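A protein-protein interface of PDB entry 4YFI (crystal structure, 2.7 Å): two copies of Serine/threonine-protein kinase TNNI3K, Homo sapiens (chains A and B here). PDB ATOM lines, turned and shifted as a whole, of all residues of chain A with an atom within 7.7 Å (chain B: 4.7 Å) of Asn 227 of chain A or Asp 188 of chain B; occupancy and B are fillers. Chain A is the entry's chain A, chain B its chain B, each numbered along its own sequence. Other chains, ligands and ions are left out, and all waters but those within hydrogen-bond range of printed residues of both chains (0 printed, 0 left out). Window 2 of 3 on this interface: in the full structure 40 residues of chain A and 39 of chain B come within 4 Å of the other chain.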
ATOM      1  N   GLY A 226       9.810  23.710   5.776  1.00  0.00           N
ATOM      2  CA  GLY A 226      10.898  22.860   6.273  1.00  0.00           C
ATOM      3  C   GLY A 226      10.681  21.381   5.975  1.00  0.00           C
ATOM      4  O   GLY A 226       9.900  21.055   5.077  1.00  0.00           O
ATOM      5  N   ASN A 227      11.385  20.475   6.671  1.00  0.00           N
ATOM      6  CA  ASN A 227      12.521  20.816   7.525  1.00  0.00           C
ATOM      7  C   ASN A 227      13.785  21.021   6.689  1.00  0.00           C
ATOM      8  O   ASN A 227      14.082  20.268   5.767  1.00  0.00           O
ATOM      9  CB  ASN A 227      12.778  19.752   8.590  1.00  0.00           C
ATOM     10  CG  ASN A 227      13.750  20.234   9.670  1.00  0.00           C
ATOM     11  OD1 ASN A 227      14.957  20.011   9.586  1.00  0.00           O
ATOM     12  ND2 ASN A 227      13.227  20.922  10.677  1.00  0.00           N
ATOM     13  N   LEU A 228      14.532  22.045   7.066  1.00  0.00           N
ATOM     14  CA  LEU A 228      15.615  22.601   6.266  1.00  0.00           C
ATOM     15  C   LEU A 228      16.873  21.766   6.322  1.00  0.00           C
ATOM     16  O   LEU A 228      17.647  21.729   5.378  1.00  0.00           O
ATOM     17  CB  LEU A 228      15.933  24.016   6.762  1.00  0.00           C
ATOM     18  CG  LEU A 228      14.785  25.037   6.701  1.00  0.00           C
ATOM     19  CD1 LEU A 228      15.106  26.277   7.518  1.00  0.00           C
ATOM     20  CD2 LEU A 228      14.465  25.426   5.269  1.00  0.00           C
ATOM     21  N   ARG A 229      17.070  21.096   7.440  1.00  0.00           N
ATOM     22  CA  ARG A 229      18.267  20.307   7.668  1.00  0.00           C
ATOM     23  C   ARG A 229      18.479  19.250   6.594  1.00  0.00           C
ATOM     24  O   ARG A 229      19.619  18.923   6.276  1.00  0.00           O
ATOM     25  CB  ARG A 229      18.181  19.662   9.045  1.00  0.00           C
ATOM     26  CG  ARG A 229      19.398  18.882   9.483  1.00  0.00           C
ATOM     27  CD  ARG A 229      19.102  18.211  10.814  1.00  0.00           C
ATOM     28  NE  ARG A 229      18.613  19.168  11.811  1.00  0.00           N
ATOM     29  CZ  ARG A 229      19.385  19.957  12.556  1.00  0.00           C
ATOM     30  NH1 ARG A 229      18.825  20.790  13.417  1.00  0.00           N
ATOM     31  NH2 ARG A 229      20.708  19.930  12.448  1.00  0.00           N
ATOM     32  N   TRP A 230      17.393  18.724   6.036  1.00  0.00           N
ATOM     33  CA  TRP A 230      17.483  17.669   5.031  1.00  0.00           C
ATOM     34  C   TRP A 230      17.277  18.152   3.595  1.00  0.00           C
ATOM     35  O   TRP A 230      17.344  17.341   2.682  1.00  0.00           O
ATOM     36  CB  TRP A 230      16.460  16.582   5.330  1.00  0.00           C
ATOM     37  CG  TRP A 230      16.793  15.754   6.491  1.00  0.00           C
ATOM     38  CD1 TRP A 230      17.488  14.606   6.476  1.00  0.00           C
ATOM     39  CD2 TRP A 230      16.417  15.987   7.858  1.00  0.00           C
ATOM     40  NE1 TRP A 230      17.588  14.092   7.746  1.00  0.00           N
ATOM     41  CE2 TRP A 230      16.938  14.921   8.616  1.00  0.00           C
ATOM     42  CE3 TRP A 230      15.679  16.985   8.510  1.00  0.00           C
ATOM     43  CZ2 TRP A 230      16.754  14.820  10.004  1.00  0.00           C
ATOM     44  CZ3 TRP A 230      15.503  16.895   9.891  1.00  0.00           C
ATOM     45  CH2 TRP A 230      16.038  15.817  10.622  1.00  0.00           C
ATOM     46  N   MET A 231      17.018  19.444   3.390  1.00  0.00           N
ATOM     47  CA  MET A 231      16.779  19.984   2.041  1.00  0.00           C
ATOM     48  C   MET A 231      17.990  19.986   1.130  1.00  0.00           C
ATOM     49  O   MET A 231      19.121  20.161   1.575  1.00  0.00           O
ATOM     50  CB  MET A 231      16.329  21.434   2.110  1.00  0.00           C
ATOM     51  CG  MET A 231      14.902  21.632   2.530  1.00  0.00           C
ATOM     52  SD  MET A 231      14.362  23.312   2.211  1.00  0.00           S
ATOM     53  CE  MET A 231      12.621  23.121   2.632  1.00  0.00           C
ATOM     54  N   ALA A 232      17.722  19.864  -0.161  1.00  0.00           N
ATOM     55  CA  ALA A 232      18.730  20.063  -1.191  1.00  0.00           C
ATOM     56  C   ALA A 232      19.019  21.549  -1.306  1.00  0.00           C
ATOM     57  O   ALA A 232      18.090  22.349  -1.255  1.00  0.00           O
ATOM     58  CB  ALA A 232      18.236  19.537  -2.526  1.00  0.00           C
ATOM     59  N   HIS B 186       8.900  13.635  -3.555  1.00  0.00           N
ATOM     60  CA  HIS B 186       8.441  13.706  -2.168  1.00  0.00           C
ATOM     61  C   HIS B 186       8.618  15.115  -1.587  1.00  0.00           C
ATOM     62  O   HIS B 186       7.694  15.642  -0.981  1.00  0.00           O
ATOM     63  CB  HIS B 186       9.188  12.679  -1.326  1.00  0.00           C
ATOM     64  CG  HIS B 186       8.640  12.493   0.054  1.00  0.00           C
ATOM     65  ND1 HIS B 186       9.017  13.283   1.116  1.00  0.00           N
ATOM     66  CD2 HIS B 186       7.785  11.574   0.559  1.00  0.00           C
ATOM     67  CE1 HIS B 186       8.399  12.879   2.211  1.00  0.00           C
ATOM     68  NE2 HIS B 186       7.652  11.836   1.902  1.00  0.00           N
ATOM     69  N   ARG B 187       9.812  15.689  -1.780  1.00  0.00           N
ATOM     70  CA  ARG B 187      10.208  17.061  -1.343  1.00  0.00           C
ATOM     71  C   ARG B 187      10.390  17.298   0.151  1.00  0.00           C
ATOM     72  O   ARG B 187      10.669  18.408   0.566  1.00  0.00           O
ATOM     73  CB  ARG B 187       9.256  18.141  -1.866  1.00  0.00           C
ATOM     74  CG  ARG B 187       9.269  18.356  -3.366  1.00  0.00           C
ATOM     75  CD  ARG B 187       8.918  19.801  -3.703  1.00  0.00           C
ATOM     76  NE  ARG B 187       7.704  20.250  -3.003  1.00  0.00           N
ATOM     77  CZ  ARG B 187       7.252  21.503  -2.983  1.00  0.00           C
ATOM     78  NH1 ARG B 187       7.905  22.464  -3.634  1.00  0.00           N
ATOM     79  NH2 ARG B 187       6.143  21.802  -2.305  1.00  0.00           N
ATOM     80  N   ASP B 188      10.206  16.274   0.960  1.00  0.00           N
ATOM     81  CA  ASP B 188      10.342  16.401   2.398  1.00  0.00           C
ATOM     82  C   ASP B 188      10.884  15.127   3.030  1.00  0.00           C
ATOM     83  O   ASP B 188      10.568  14.810   4.177  1.00  0.00           O
ATOM     84  CB  ASP B 188       8.982  16.753   3.007  1.00  0.00           C
ATOM     85  CG  ASP B 188       9.098  17.355   4.412  1.00  0.00           C
ATOM     86  OD1 ASP B 188      10.124  18.015   4.740  1.00  0.00           O
ATOM     87  OD2 ASP B 188       8.148  17.162   5.187  1.00  0.00           O
ATOM     88  N   LEU B 189      11.717  14.410   2.293  1.00  0.00           N
ATOM     89  CA  LEU B 189      12.235  13.160   2.769  1.00  0.00           C
ATOM     90  C   LEU B 189      13.217  13.410   3.925  1.00  0.00           C
ATOM     91  O   LEU B 189      14.218  14.124   3.773  1.00  0.00           O
ATOM     92  CB  LEU B 189      12.913  12.393   1.628  1.00  0.00           C
ATOM     93  CG  LEU B 189      13.475  11.008   1.985  1.00  0.00           C
ATOM     94  CD1 LEU B 189      12.363  10.072   2.399  1.00  0.00           C
ATOM     95  CD2 LEU B 189      14.235  10.393   0.818  1.00  0.00           C
ATOM     96  N   ASN B 190      12.910  12.832   5.077  1.00  0.00           N
ATOM     97  CA  ASN B 190      13.783  12.898   6.233  1.00  0.00           C
ATOM     98  C   ASN B 190      13.374  11.805   7.203  1.00  0.00           C
ATOM     99  O   ASN B 190      12.354  11.144   6.980  1.00  0.00           O
ATOM    100  CB  ASN B 190      13.673  14.250   6.904  1.00  0.00           C
ATOM    101  CG  ASN B 190      12.285  14.525   7.426  1.00  0.00           C
ATOM    102  OD1 ASN B 190      11.666  13.668   8.047  1.00  0.00           O
ATOM    103  ND2 ASN B 190      11.783  15.719   7.171  1.00  0.00           N
ATOM    104  N   ASN B 193       9.842  11.315   8.435  1.00  0.00           N
ATOM    105  CA  ASN B 193       8.925  10.768   7.433  1.00  0.00           C
ATOM    106  C   ASN B 193       9.330   9.400   6.870  1.00  0.00           C
ATOM    107  O   ASN B 193       8.860   8.976   5.814  1.00  0.00           O
ATOM    108  CB  ASN B 193       8.769  11.786   6.315  1.00  0.00           C
ATOM    109  CG  ASN B 193       8.238  13.098   6.826  1.00  0.00           C
ATOM    110  OD1 ASN B 193       7.695  13.164   7.936  1.00  0.00           O
ATOM    111  ND2 ASN B 193       8.400  14.163   6.033  1.00  0.00           N
ATOM    112  N   GLU B 209       4.172  17.735   1.304  1.00  0.00           N
ATOM    113  CA  GLU B 209       4.953  18.653   0.477  1.00  0.00           C
ATOM    114  C   GLU B 209       5.178  18.095  -0.932  1.00  0.00           C
ATOM    115  O   GLU B 209       5.947  18.670  -1.705  1.00  0.00           O
ATOM    116  CB  GLU B 209       6.323  18.935   1.131  1.00  0.00           C
ATOM    117  CG  GLU B 209       6.279  19.595   2.515  1.00  0.00           C
ATOM    118  CD  GLU B 209       5.686  20.995   2.507  1.00  0.00           C
ATOM    119  OE1 GLU B 209       5.959  21.775   1.568  1.00  0.00           O
ATOM    120  OE2 GLU B 209       4.948  21.325   3.453  1.00  0.00           O
ATOM    121  N   PRO B 270      18.258  24.076  12.310  1.00  0.00           N
ATOM    122  CA  PRO B 270      17.997  23.708  10.915  1.00  0.00           C
ATOM    123  C   PRO B 270      18.536  24.687   9.861  1.00  0.00           C
ATOM    124  O   PRO B 270      19.235  24.284   8.936  1.00  0.00           O
ATOM    125  CB  PRO B 270      16.460  23.627  10.865  1.00  0.00           C
ATOM    126  CG  PRO B 270      16.075  23.190  12.236  1.00  0.00           C
ATOM    127  CD  PRO B 270      17.113  23.742  13.184  1.00  0.00           C
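The side-chain carboxylate (OD1) of Asp 188 of chain B lies close to the backbone carbonyl oxygen (O) of Gly 226 of chain A, 3.1 Å away. The backbone NH of Asn 227 of chain A lies within hydrogen-bond range of the side-chain carboxylate of Asp 188 of chain B (3.4 Å).
ND1 of His 186 of chain B lies close to N of Asp 188 of chain B, at 3.2 Å. The backbone carbonyl oxygen (O) of Asp 188 of chain B lies within hydrogen-bond range of the side-chain amide nitrogen (ND2) of Asn 193 of chain B (2.9 Å). The side-chain amide oxygen (OD1) of Asn 190 of chain B lies within hydrogen-bond range of the backbone NH (N) of Asn 193 of chain B. N of Arg 229 of chain A lies within hydrogen-bond range of OD1 of Asn 227 of chain A (3.2 Å). O of Asp 188 of chain B sits at hydrogen-bond distance from ND2 of Asn 190 of chain B, at 3.4 Å. A ring nitrogen (ND1) of His 186 of chain B lies within hydrogen-bond range of the backbone NH (N) of Leu 189 of chain B, 3.2 Å away.
Among the printed residues, pairs that only touch across the chains: Asn 227 of chain A with Pro 270 of chain B (3.96 Å), Leu 228 of chain A with Pro 270 of chain B (3.96 Å), Arg 229 of chain A with Pro 270 of chain B (3.4 Å), Trp 230 of chain A with Leu 189 of chain B (3.7 Å) and Trp 230 of chain A with Asn 190 of chain B (3.4 Å).
Asn 227 of chain A touches two residues of chain B. Of the printed residues of chain A, Leu 189 of chain B touches Trp 230. Of the printed residues of chain B, Arg 229 of chain A touches Pro 270. Printed residues of chain B within 4 Å of Leu 228 of chain A: Pro 270. Printed residues of chain A within 4 Å of Asn 190 of chain B: Trp 230. Met 231 of chain A touches none of the printed residues of chain B. His 186 of chain B touches none of the printed residues of chain A.
Of the 7 printed residues of chain A, 5 touch a printed residue of chain B. Hydrophobic or aromatic side chains of chain A that line the printed part of chain B: Leu 228 and Trp 230. Among the printed residues, 7 pairs touch across the chains.
No position is printed for both chains.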
